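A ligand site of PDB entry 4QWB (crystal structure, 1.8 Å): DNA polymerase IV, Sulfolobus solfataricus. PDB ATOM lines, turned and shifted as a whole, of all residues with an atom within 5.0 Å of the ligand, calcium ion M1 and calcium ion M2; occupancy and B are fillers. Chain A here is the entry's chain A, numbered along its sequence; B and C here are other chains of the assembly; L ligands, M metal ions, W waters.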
ATOM      1  N   PHE A   5       3.130  13.420  23.773  1.00  0.00           N
ATOM      2  CA  PHE A   5       1.774  13.552  23.263  1.00  0.00           C
ATOM      3  C   PHE A   5       0.798  12.986  24.296  1.00  0.00           C
ATOM      4  O   PHE A   5       1.042  11.913  24.849  1.00  0.00           O
ATOM      5  CB  PHE A   5       1.681  12.788  21.965  1.00  0.00           C
ATOM      6  CG  PHE A   5       0.291  12.611  21.427  1.00  0.00           C
ATOM      7  CD1 PHE A   5      -0.368  13.663  20.780  1.00  0.00           C
ATOM      8  CD2 PHE A   5      -0.345  11.369  21.492  1.00  0.00           C
ATOM      9  CE1 PHE A   5      -1.635  13.480  20.263  1.00  0.00           C
ATOM     10  CE2 PHE A   5      -1.605  11.191  20.954  1.00  0.00           C
ATOM     11  CZ  PHE A   5      -2.256  12.252  20.341  1.00  0.00           C
ATOM     12  N   ASP A   7      -3.336  11.996  24.919  1.00  0.00           N
ATOM     13  CA  ASP A   7      -4.590  11.715  24.233  1.00  0.00           C
ATOM     14  C   ASP A   7      -5.538  11.196  25.320  1.00  0.00           C
ATOM     15  O   ASP A   7      -5.230  10.182  25.941  1.00  0.00           O
ATOM     16  CB  ASP A   7      -4.359  10.663  23.144  1.00  0.00           C
ATOM     17  CG  ASP A   7      -5.611  10.358  22.297  1.00  0.00           C
ATOM     18  OD1 ASP A   7      -6.739  10.337  22.817  1.00  0.00           O
ATOM     19  OD2 ASP A   7      -5.480  10.089  21.068  1.00  0.00           O
ATOM     20  N   PHE A   8      -6.645  11.882  25.584  1.00  0.00           N
ATOM     21  CA  PHE A   8      -7.503  11.524  26.732  1.00  0.00           C
ATOM     22  C   PHE A   8      -8.261  10.231  26.386  1.00  0.00           C
ATOM     23  O   PHE A   8      -8.689  10.078  25.255  1.00  0.00           O
ATOM     24  CB  PHE A   8      -8.504  12.641  27.133  1.00  0.00           C
ATOM     25  CG  PHE A   8      -7.892  14.028  27.254  1.00  0.00           C
ATOM     26  CD1 PHE A   8      -6.550  14.216  27.531  1.00  0.00           C
ATOM     27  CD2 PHE A   8      -8.698  15.160  27.116  1.00  0.00           C
ATOM     28  CE1 PHE A   8      -6.019  15.496  27.636  1.00  0.00           C
ATOM     29  CE2 PHE A   8      -8.171  16.442  27.230  1.00  0.00           C
ATOM     30  CZ  PHE A   8      -6.831  16.605  27.491  1.00  0.00           C
ATOM     31  N   ASP A   9      -8.426   9.317  27.349  1.00  0.00           N
ATOM     32  CA  ASP A   9      -9.111   8.028  27.091  1.00  0.00           C
ATOM     33  C   ASP A   9     -10.637   8.192  26.994  1.00  0.00           C
ATOM     34  O   ASP A   9     -11.239   8.940  27.761  1.00  0.00           O
ATOM     35  CB  ASP A   9      -8.825   7.004  28.200  1.00  0.00           C
ATOM     36  CG  ASP A   9      -7.333   6.689  28.391  1.00  0.00           C
ATOM     37  OD1 ASP A   9      -6.586   6.543  27.405  1.00  0.00           O
ATOM     38  OD2 ASP A   9      -6.920   6.531  29.558  1.00  0.00           O
ATOM     39  N   TYR A  10     -11.236   7.493  26.022  1.00  0.00           N
ATOM     40  CA  TYR A  10     -12.688   7.400  25.861  1.00  0.00           C
ATOM     41  C   TYR A  10     -13.384   8.720  26.179  1.00  0.00           C
ATOM     42  O   TYR A  10     -14.369   8.717  26.880  1.00  0.00           O
ATOM     43  CB  TYR A  10     -13.247   6.280  26.779  1.00  0.00           C
ATOM     44  CG  TYR A  10     -12.623   4.936  26.482  1.00  0.00           C
ATOM     45  CD1 TYR A  10     -12.907   4.271  25.310  1.00  0.00           C
ATOM     46  CD2 TYR A  10     -11.720   4.354  27.372  1.00  0.00           C
ATOM     47  CE1 TYR A  10     -12.328   3.052  25.014  1.00  0.00           C
ATOM     48  CE2 TYR A  10     -11.129   3.124  27.074  1.00  0.00           C
ATOM     49  CZ  TYR A  10     -11.434   2.489  25.895  1.00  0.00           C
ATOM     50  OH  TYR A  10     -10.872   1.269  25.558  1.00  0.00           O
ATOM     51  N   PHE A  11     -12.886   9.829  25.631  1.00  0.00           N
ATOM     52  CA  PHE A  11     -13.030  11.119  26.309  1.00  0.00           C
ATOM     53  C   PHE A  11     -14.446  11.547  26.680  1.00  0.00           C
ATOM     54  O   PHE A  11     -14.708  11.765  27.867  1.00  0.00           O
ATOM     55  CB  PHE A  11     -12.279  12.258  25.580  1.00  0.00           C
ATOM     56  CG  PHE A  11     -12.328  13.582  26.311  1.00  0.00           C
ATOM     57  CD1 PHE A  11     -11.920  13.677  27.641  1.00  0.00           C
ATOM     58  CD2 PHE A  11     -12.777  14.730  25.682  1.00  0.00           C
ATOM     59  CE1 PHE A  11     -11.981  14.883  28.321  1.00  0.00           C
ATOM     60  CE2 PHE A  11     -12.824  15.945  26.354  1.00  0.00           C
ATOM     61  CZ  PHE A  11     -12.431  16.026  27.671  1.00  0.00           C
ATOM     62  N   TYR A  12     -15.354  11.640  25.711  1.00  0.00           N
ATOM     63  CA  TYR A  12     -16.701  12.116  26.032  1.00  0.00           C
ATOM     64  C   TYR A  12     -17.397  11.195  27.026  1.00  0.00           C
ATOM     65  O   TYR A  12     -18.064  11.664  27.945  1.00  0.00           O
ATOM     66  CB  TYR A  12     -17.577  12.217  24.793  1.00  0.00           C
ATOM     67  CG  TYR A  12     -17.203  13.299  23.806  1.00  0.00           C
ATOM     68  CD1 TYR A  12     -16.076  14.103  23.976  1.00  0.00           C
ATOM     69  CD2 TYR A  12     -17.969  13.474  22.651  1.00  0.00           C
ATOM     70  CE1 TYR A  12     -15.752  15.083  23.030  1.00  0.00           C
ATOM     71  CE2 TYR A  12     -17.641  14.432  21.702  1.00  0.00           C
ATOM     72  CZ  TYR A  12     -16.542  15.238  21.915  1.00  0.00           C
ATOM     73  OH  TYR A  12     -16.223  16.186  20.964  1.00  0.00           O
ATOM     74  N   ALA A  44     -21.009   9.127  18.764  1.00  0.00           N
ATOM     75  CA  ALA A  44     -19.828   9.977  18.842  1.00  0.00           C
ATOM     76  C   ALA A  44     -18.669   9.191  19.417  1.00  0.00           C
ATOM     77  O   ALA A  44     -17.574   9.205  18.872  1.00  0.00           O
ATOM     78  CB  ALA A  44     -20.114  11.194  19.703  1.00  0.00           C
ATOM     79  N   THR A  45     -18.920   8.507  20.536  1.00  0.00           N
ATOM     80  CA  THR A  45     -17.955   7.563  21.094  1.00  0.00           C
ATOM     81  C   THR A  45     -18.651   6.642  22.088  1.00  0.00           C
ATOM     82  O   THR A  45     -19.802   6.821  22.430  1.00  0.00           O
ATOM     83  CB  THR A  45     -16.747   8.285  21.759  1.00  0.00           C
ATOM     84  OG1 THR A  45     -15.632   7.396  21.849  1.00  0.00           O
ATOM     85  CG2 THR A  45     -17.090   8.819  23.148  1.00  0.00           C
ATOM     86  N   ALA A  46     -17.909   5.630  22.546  1.00  0.00           N
ATOM     87  CA  ALA A  46     -18.383   4.736  23.572  1.00  0.00           C
ATOM     88  C   ALA A  46     -17.198   4.353  24.438  1.00  0.00           C
ATOM     89  O   ALA A  46     -16.051   4.415  23.993  1.00  0.00           O
ATOM     90  CB  ALA A  46     -19.014   3.501  22.951  1.00  0.00           C
ATOM     91  N   ARG A  51     -17.447  -0.540  23.628  1.00  0.00           N
ATOM     92  CA  ARG A  51     -16.626  -0.627  22.443  1.00  0.00           C
ATOM     93  C   ARG A  51     -16.108  -2.033  22.185  1.00  0.00           C
ATOM     94  O   ARG A  51     -15.975  -2.425  21.037  1.00  0.00           O
ATOM     95  CB  ARG A  51     -15.473   0.364  22.503  1.00  0.00           C
ATOM     96  CG  ARG A  51     -15.225   1.005  21.159  1.00  0.00           C
ATOM     97  CD  ARG A  51     -15.031   2.494  21.296  1.00  0.00           C
ATOM     98  NE  ARG A  51     -13.621   2.794  21.268  1.00  0.00           N
ATOM     99  CZ  ARG A  51     -13.062   3.939  21.636  1.00  0.00           C
ATOM    100  NH1 ARG A  51     -13.784   4.956  22.096  1.00  0.00           N
ATOM    101  NH2 ARG A  51     -11.749   4.039  21.521  1.00  0.00           N
ATOM    102  N   ALA A  57     -17.342   4.662  17.316  1.00  0.00           N
ATOM    103  CA  ALA A  57     -17.692   5.962  16.754  1.00  0.00           C
ATOM    104  C   ALA A  57     -18.184   5.839  15.317  1.00  0.00           C
ATOM    105  O   ALA A  57     -17.634   5.063  14.524  1.00  0.00           O
ATOM    106  CB  ALA A  57     -16.512   6.918  16.836  1.00  0.00           C
ATOM    107  N   GLY A  58     -19.228   6.592  15.004  1.00  0.00           N
ATOM    108  CA  GLY A  58     -19.723   6.664  13.634  1.00  0.00           C
ATOM    109  C   GLY A  58     -20.844   5.710  13.296  1.00  0.00           C
ATOM    110  O   GLY A  58     -21.580   5.971  12.343  1.00  0.00           O
ATOM    111  N   MET A  76     -24.795  13.715  23.275  1.00  0.00           N
ATOM    112  CA  MET A  76     -23.547  14.453  23.324  1.00  0.00           C
ATOM    113  C   MET A  76     -23.791  15.819  23.936  1.00  0.00           C
ATOM    114  O   MET A  76     -24.739  16.516  23.533  1.00  0.00           O
ATOM    115  CB  MET A  76     -22.981  14.614  21.903  1.00  0.00           C
ATOM    116  CG  MET A  76     -21.522  15.059  21.877  1.00  0.00           C
ATOM    117  SD  MET A  76     -20.909  15.242  20.200  1.00  0.00           S
ATOM    118  CE  MET A  76     -21.860  16.646  19.654  1.00  0.00           C
ATOM    119  N   ILE A 104      -9.816  18.449  20.748  1.00  0.00           N
ATOM    120  CA  ILE A 104     -10.553  18.493  22.004  1.00  0.00           C
ATOM    121  C   ILE A 104      -9.921  17.592  23.081  1.00  0.00           C
ATOM    122  O   ILE A 104     -10.091  17.852  24.273  1.00  0.00           O
ATOM    123  CB  ILE A 104     -12.055  18.135  21.818  1.00  0.00           C
ATOM    124  CG1 ILE A 104     -12.859  18.551  23.064  1.00  0.00           C
ATOM    125  CG2 ILE A 104     -12.246  16.656  21.454  1.00  0.00           C
ATOM    126  CD1 ILE A 104     -14.338  18.700  22.801  1.00  0.00           C
ATOM    127  N   ASP A 105      -9.187  16.559  22.676  1.00  0.00           N
ATOM    128  CA  ASP A 105      -8.593  15.644  23.662  1.00  0.00           C
ATOM    129  C   ASP A 105      -7.095  15.315  23.467  1.00  0.00           C
ATOM    130  O   ASP A 105      -6.607  14.330  24.011  1.00  0.00           O
ATOM    131  CB  ASP A 105      -9.450  14.366  23.776  1.00  0.00           C
ATOM    132  CG  ASP A 105      -9.198  13.385  22.643  1.00  0.00           C
ATOM    133  OD1 ASP A 105      -8.828  13.811  21.535  1.00  0.00           O
ATOM    134  OD2 ASP A 105      -9.387  12.166  22.882  1.00  0.00           O
ATOM    135  N   GLU A 106      -6.369  16.175  22.739  1.00  0.00           N
ATOM    136  CA  GLU A 106      -4.968  15.940  22.464  1.00  0.00           C
ATOM    137  C   GLU A 106      -4.096  17.181  22.592  1.00  0.00           C
ATOM    138  O   GLU A 106      -4.490  18.277  22.192  1.00  0.00           O
ATOM    139  CB  GLU A 106      -4.766  15.429  21.041  1.00  0.00           C
ATOM    140  CG  GLU A 106      -5.408  14.108  20.709  1.00  0.00           C
ATOM    141  CD  GLU A 106      -5.445  13.881  19.217  1.00  0.00           C
ATOM    142  OE1 GLU A 106      -5.843  14.825  18.487  1.00  0.00           O
ATOM    143  OE2 GLU A 106      -5.103  12.784  18.751  1.00  0.00           O
ATOM    144  N   LYS A 152       2.329  10.180  18.536  1.00  0.00           N
ATOM    145  CA  LYS A 152       0.935   9.721  18.402  1.00  0.00           C
ATOM    146  C   LYS A 152       0.855   8.202  18.233  1.00  0.00           C
ATOM    147  O   LYS A 152       0.013   7.557  18.873  1.00  0.00           O
ATOM    148  CB  LYS A 152       0.227  10.407  17.218  1.00  0.00           C
ATOM    149  CG  LYS A 152      -1.176   9.873  16.966  1.00  0.00           C
ATOM    150  CD  LYS A 152      -1.931  10.723  15.963  1.00  0.00           C
ATOM    151  CE  LYS A 152      -2.722  11.848  16.621  1.00  0.00           C
ATOM    152  NZ  LYS A 152      -3.882  12.247  15.773  1.00  0.00           N
ATOM    153  N   LYS A 159      -2.759   2.630  24.397  1.00  0.00           N
ATOM    154  CA  LYS A 159      -4.121   2.901  24.836  1.00  0.00           C
ATOM    155  C   LYS A 159      -4.824   1.660  25.389  1.00  0.00           C
ATOM    156  O   LYS A 159      -4.675   0.581  24.834  1.00  0.00           O
ATOM    157  CB  LYS A 159      -4.976   3.409  23.684  1.00  0.00           C
ATOM    158  CG  LYS A 159      -4.800   4.869  23.416  1.00  0.00           C
ATOM    159  CD  LYS A 159      -5.676   5.293  22.256  1.00  0.00           C
ATOM    160  CE  LYS A 159      -5.335   6.705  21.859  1.00  0.00           C
ATOM    161  NZ  LYS A 159      -6.318   7.198  20.869  1.00  0.00           N
ATOM    162  P    DT B  12      -6.574   9.448   9.552  1.00  0.00           P
ATOM    163  OP1  DT B  12      -5.313   8.845  10.041  1.00  0.00           O
ATOM    164  OP2  DT B  12      -7.748   8.587   9.323  1.00  0.00           O
ATOM    165  O5'  DT B  12      -6.978  10.613  10.557  1.00  0.00           O
ATOM    166  C5'  DT B  12      -5.975  11.383  11.234  1.00  0.00           C
ATOM    167  C4'  DT B  12      -6.591  12.510  12.023  1.00  0.00           C
ATOM    168  O4'  DT B  12      -7.471  13.294  11.187  1.00  0.00           O
ATOM    169  C3'  DT B  12      -7.463  12.106  13.190  1.00  0.00           C
ATOM    170  O3'  DT B  12      -6.711  11.744  14.346  1.00  0.00           O
ATOM    171  C2'  DT B  12      -8.287  13.359  13.415  1.00  0.00           C
ATOM    172  C1'  DT B  12      -8.449  13.925  12.005  1.00  0.00           C
ATOM    173  N1   DT B  12      -9.786  13.708  11.400  1.00  0.00           N
ATOM    174  C2   DT B  12     -10.736  14.678  11.606  1.00  0.00           C
ATOM    175  O2   DT B  12     -10.517  15.697  12.257  1.00  0.00           O
ATOM    176  N3   DT B  12     -11.947  14.433  11.018  1.00  0.00           N
ATOM    177  C4   DT B  12     -12.304  13.328  10.276  1.00  0.00           C
ATOM    178  O4   DT B  12     -13.433  13.246   9.790  1.00  0.00           O
ATOM    179  C5   DT B  12     -11.258  12.336  10.106  1.00  0.00           C
ATOM    180  C7   DT B  12     -11.551  11.093   9.318  1.00  0.00           C
ATOM    181  C6   DT B  12     -10.075  12.568  10.685  1.00  0.00           C
ATOM    182  N1  DOC B  13     -12.158  13.694  15.229  1.00  0.00           N
ATOM    183  C2  DOC B  13     -13.472  14.079  14.926  1.00  0.00           C
ATOM    184  N3  DOC B  13     -14.187  13.351  14.035  1.00  0.00           N
ATOM    185  C4  DOC B  13     -13.628  12.282  13.453  1.00  0.00           C
ATOM    186  C5  DOC B  13     -12.301  11.866  13.759  1.00  0.00           C
ATOM    187  C6  DOC B  13     -11.604  12.591  14.643  1.00  0.00           C
ATOM    188  O2  DOC B  13     -13.946  15.086  15.473  1.00  0.00           O
ATOM    189  N4  DOC B  13     -14.368  11.592  12.586  1.00  0.00           N
ATOM    190  C1' DOC B  13     -11.404  14.522  16.187  1.00  0.00           C
ATOM    191  C2' DOC B  13     -11.571  14.109  17.648  1.00  0.00           C
ATOM    192  C3' DOC B  13     -10.275  13.397  17.969  1.00  0.00           C
ATOM    193  C4' DOC B  13      -9.269  14.102  17.068  1.00  0.00           C
ATOM    194  O4' DOC B  13     -10.024  14.422  15.876  1.00  0.00           O
ATOM    195  C5' DOC B  13      -8.069  13.267  16.718  1.00  0.00           C
ATOM    196  O5' DOC B  13      -8.481  12.057  16.083  1.00  0.00           O
ATOM    197  P   DOC B  13      -7.414  10.994  15.582  1.00  0.00           P
ATOM    198  OP1 DOC B  13      -6.391  10.800  16.640  1.00  0.00           O
ATOM    199  OP2 DOC B  13      -8.180   9.849  15.057  1.00  0.00           O
ATOM    200  P    DG C   5     -25.328  10.734   9.286  1.00  0.00           P
ATOM    201  OP1  DG C   5     -26.620  11.202   8.721  1.00  0.00           O
ATOM    202  OP2  DG C   5     -24.073  10.903   8.519  1.00  0.00           O
ATOM    203  O5'  DG C   5     -25.112  11.416  10.705  1.00  0.00           O
ATOM    204  C5'  DG C   5     -26.038  11.227  11.788  1.00  0.00           C
ATOM    205  C4'  DG C   5     -25.851  12.344  12.791  1.00  0.00           C
ATOM    206  O4'  DG C   5     -24.672  12.095  13.583  1.00  0.00           O
ATOM    207  C3'  DG C   5     -25.620  13.715  12.167  1.00  0.00           C
ATOM    208  O3'  DG C   5     -26.107  14.698  13.075  1.00  0.00           O
ATOM    209  C2'  DG C   5     -24.106  13.757  11.998  1.00  0.00           C
ATOM    210  C1'  DG C   5     -23.614  12.976  13.206  1.00  0.00           C
ATOM    211  N9   DG C   5     -22.420  12.167  13.026  1.00  0.00           N
ATOM    212  C8   DG C   5     -22.217  11.172  12.100  1.00  0.00           C
ATOM    213  N7   DG C   5     -21.064  10.566  12.239  1.00  0.00           N
ATOM    214  C5   DG C   5     -20.486  11.177  13.340  1.00  0.00           C
ATOM    215  C6   DG C   5     -19.245  10.936  13.976  1.00  0.00           C
ATOM    216  O6   DG C   5     -18.372  10.110  13.685  1.00  0.00           O
ATOM    217  N1   DG C   5     -19.055  11.777  15.069  1.00  0.00           N
ATOM    218  C2   DG C   5     -19.951  12.724  15.496  1.00  0.00           C
ATOM    219  N2   DG C   5     -19.592  13.445  16.573  1.00  0.00           N
ATOM    220  N3   DG C   5     -21.121  12.952  14.928  1.00  0.00           N
ATOM    221  C4   DG C   5     -21.322  12.147  13.853  1.00  0.00           C
ATOM    222  P    DG C   6     -26.403  16.181  12.575  1.00  0.00           P
ATOM    223  OP1  DG C   6     -27.340  16.810  13.535  1.00  0.00           O
ATOM    224  OP2  DG C   6     -26.733  16.124  11.122  1.00  0.00           O
ATOM    225  O5'  DG C   6     -25.015  16.902  12.790  1.00  0.00           O
ATOM    226  C5'  DG C   6     -24.618  17.225  14.118  1.00  0.00           C
ATOM    227  C4'  DG C   6     -23.137  17.483  14.167  1.00  0.00           C
ATOM    228  O4'  DG C   6     -22.384  16.328  13.770  1.00  0.00           O
ATOM    229  C3'  DG C   6     -22.657  18.631  13.274  1.00  0.00           C
ATOM    230  O3'  DG C   6     -22.218  19.597  14.226  1.00  0.00           O
ATOM    231  C2'  DG C   6     -21.569  18.011  12.422  1.00  0.00           C
ATOM    232  C1'  DG C   6     -21.169  16.825  13.288  1.00  0.00           C
ATOM    233  N9   DG C   6     -20.414  15.727  12.685  1.00  0.00           N
ATOM    234  C8   DG C   6     -20.779  14.893  11.649  1.00  0.00           C
ATOM    235  N7   DG C   6     -19.876  13.990  11.382  1.00  0.00           N
ATOM    236  C5   DG C   6     -18.872  14.224  12.300  1.00  0.00           C
ATOM    237  C6   DG C   6     -17.631  13.563  12.503  1.00  0.00           C
ATOM    238  O6   DG C   6     -17.165  12.607  11.882  1.00  0.00           O
ATOM    239  N1   DG C   6     -16.910  14.127  13.555  1.00  0.00           N
ATOM    240  C2   DG C   6     -17.332  15.192  14.310  1.00  0.00           C
ATOM    241  N2   DG C   6     -16.499  15.599  15.285  1.00  0.00           N
ATOM    242  N3   DG C   6     -18.487  15.811  14.144  1.00  0.00           N
ATOM    243  C4   DG C   6     -19.192  15.286  13.122  1.00  0.00           C
HETATM  244  O1  LIG L   1     -11.486   6.867  22.334  1.00  0.00           O
HETATM  245  P1  LIG L   1     -11.980   8.300  22.393  1.00  0.00           P
HETATM  246  O2  LIG L   1     -11.121   9.240  23.195  1.00  0.00           O
HETATM  247  O3  LIG L   1     -13.443   8.382  22.751  1.00  0.00           O
HETATM  248  O4  LIG L   1     -11.969   8.764  20.849  1.00  0.00           O
HETATM  249  P2  LIG L   1     -10.914   9.698  20.063  1.00  0.00           P
HETATM  250  O5  LIG L   1      -9.607   9.825  20.792  1.00  0.00           O
HETATM  251  O6  LIG L   1     -10.909   9.152  18.655  1.00  0.00           O
HETATM  252  O7  LIG L   1     -11.653  11.117  19.952  1.00  0.00           O
HETATM  253  C1  LIG L   1     -11.834  12.002  21.042  1.00  0.00           C
HETATM  254  C2  LIG L   1     -13.295  12.401  21.155  1.00  0.00           C
HETATM  255  O8  LIG L   1     -13.738  13.096  19.980  1.00  0.00           O
HETATM  256  C3  LIG L   1     -14.271  11.248  21.340  1.00  0.00           C
HETATM  257  O9  LIG L   1     -14.405  10.898  22.731  1.00  0.00           O
HETATM  258  C4  LIG L   1     -15.549  11.792  20.748  1.00  0.00           C
HETATM  259  C5  LIG L   1     -15.084  12.781  19.692  1.00  0.00           C
HETATM  260  N1  LIG L   1     -15.240  12.098  18.422  1.00  0.00           N
HETATM  261  C6  LIG L   1     -16.432  12.239  17.689  1.00  0.00           C
HETATM  262  O10 LIG L   1     -17.331  12.983  18.093  1.00  0.00           O
HETATM  263  N2  LIG L   1     -16.599  11.584  16.519  1.00  0.00           N
HETATM  264  C7  LIG L   1     -15.625  10.761  16.057  1.00  0.00           C
HETATM  265  N3  LIG L   1     -15.788  10.104  14.879  1.00  0.00           N
HETATM  266  C8  LIG L   1     -14.458  10.606  16.773  1.00  0.00           C
HETATM  267  C9  LIG L   1     -14.280  11.277  17.965  1.00  0.00           C
HETATM  268 CA    CA M   1      -9.018   9.981  22.948  1.00  0.00          CA
HETATM  269 CA    CA M   2      -6.156  10.724  18.956  1.00  0.00          CA
HETATM  270  O   HOH W   1     -17.342  15.738  18.449  1.00  0.00           O
HETATM  271  O   HOH W   2      -8.009  11.769  19.854  1.00  0.00           O
HETATM  272  O   HOH W   3      -9.453   6.076  20.790  1.00  0.00           O
HETATM  273  O   HOH W   4      -7.684   8.820  19.036  1.00  0.00           O
HETATM  274  O   HOH W   5      -8.198   7.710  23.097  1.00  0.00           O
HETATM  275  O   HOH W   6     -10.487   6.295  18.325  1.00  0.00           O
HETATM  276  O   HOH W   7      -9.712   5.924  24.163  1.00  0.00           O
HETATM  277  O   HOH W   8     -14.768   7.862  19.368  1.00  0.00           O
HETATM  278  O   HOH W   9     -13.512   8.253  14.424  1.00  0.00           O
HETATM  279  O   HOH W  10      -4.505   9.262  18.235  1.00  0.00           O
HETATM  280  O   HOH W  11     -10.832   9.475  15.932  1.00  0.00           O
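A nitrogen (N3) of the ligand is in hydrogen-bond range of O6 of DG 5 of chain C (2.8 Å). O2 of the ligand sits close to N of Tyr 10 (3.3 Å). The backbone NH (N) of Phe 11 sits at hydrogen-bond distance from an oxygen (O3) of the ligand (3.3 Å). N of Tyr 12 of chain A lies within hydrogen-bond range of O9 of the ligand (3.2 Å). NH2 of Arg 51 lies within salt-bridge range of O1 of the ligand (3.0 Å). N4 of DOC 13 of chain B is in hydrogen-bond range of N3 of the ligand. OG1 of Thr 45 is in hydrogen-bond range of O3 of the ligand (2.6 Å).
The backbone carbonyl oxygen of Ala 46 lies within hydrogen-bond range of the guanidinium group of Arg 51, at 3.0 Å. NZ of Lys 152 sits close to OP1 of DOC 13 of chain B, 3.0 Å away. NZ of Lys 159 sits close to OD2 of Asp 7, at 3.0 Å. O2 of DOC 13 of chain B sits close to N2 of DG 6 of chain C, at 2.6 Å. OE2 of Glu 106 lies close to NZ of Lys 152. The side-chain hydroxyl (OG1) of Thr 45 sits at hydrogen-bond distance from the guanidinium group (NH1) of Arg 51.
The backbone carbonyl oxygen (O) of Ala 44 sits close to a nitrogen (N2) of the ligand (3.5 Å). Asp 9 touches the ligand (C to O2, 3.97 Å). Ala 57 touches the ligand (CB to N3, 3.8 Å). DG 6 of chain C touches the ligand. Within 4 Å of the ligand: Asp 7, Phe 8, Asp 9, Tyr 10, Phe 11, Tyr 12 of chain A, Ala 44, Thr 45, Arg 51, Ala 57, Asp 105, DOC 13 of chain B, DG 5 of chain C and DG 6 of chain C.
Within 4 Å of calcium ion M1: Asp 7, Phe 8 and Asp 105. The nearest printed residue that does not touch calcium ion M1 is Lys 159 (4.4 Å).
Calcium ion M1 is bound by OD2 of Asp 105 (2.2 Å), O5 of the ligand (2.2 Å), O2 of the ligand (2.2 Å), OD1 of Asp 7 (2.3 Å), O of Phe 8 (2.3 Å) and water W5 (2.4 Å). Calcium ion M1 has six donor atoms within binding distance.
Calcium ion M2 is bound by OD2 of Asp 7 (2.3 Å), water W2 (2.3 Å), water W10 (2.3 Å), OE2 of Glu 106 (2.3 Å), OP1 of DOC 13 of chain B (2.3 Å) and water W4 (2.4 Å).
Water W5 bridges the side-chain amino group of Lys 159 (3.0 Å) and an oxygen (O1) of the ligand (3.5 Å). Water W4 lies within hydrogen-bond range of NZ of Lys 159 (2.8 Å) and O6 of the ligand (3.3 Å). Water W3 lies within hydrogen-bond range of an oxygen (O1) of the ligand (2.7 Å), the guanidinium group of Arg 51 (3.2 Å) and the side-chain amino group of Lys 159 (3.3 Å). Water W7 bridges O1 of the ligand (2.7 Å) and N of Tyr 10 (2.9 Å). Water W11 lies within hydrogen-bond range of an oxygen (O6) of the ligand (2.7 Å) and OP2 of DOC 13 of chain B (2.8 Å). Water W1 lies within hydrogen-bond range of an oxygen (O10) of the ligand (2.8 Å), the side-chain hydroxyl (OH) of Tyr 12 of chain A (2.8 Å) and N2 of DG 6 of chain C (3.3 Å).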
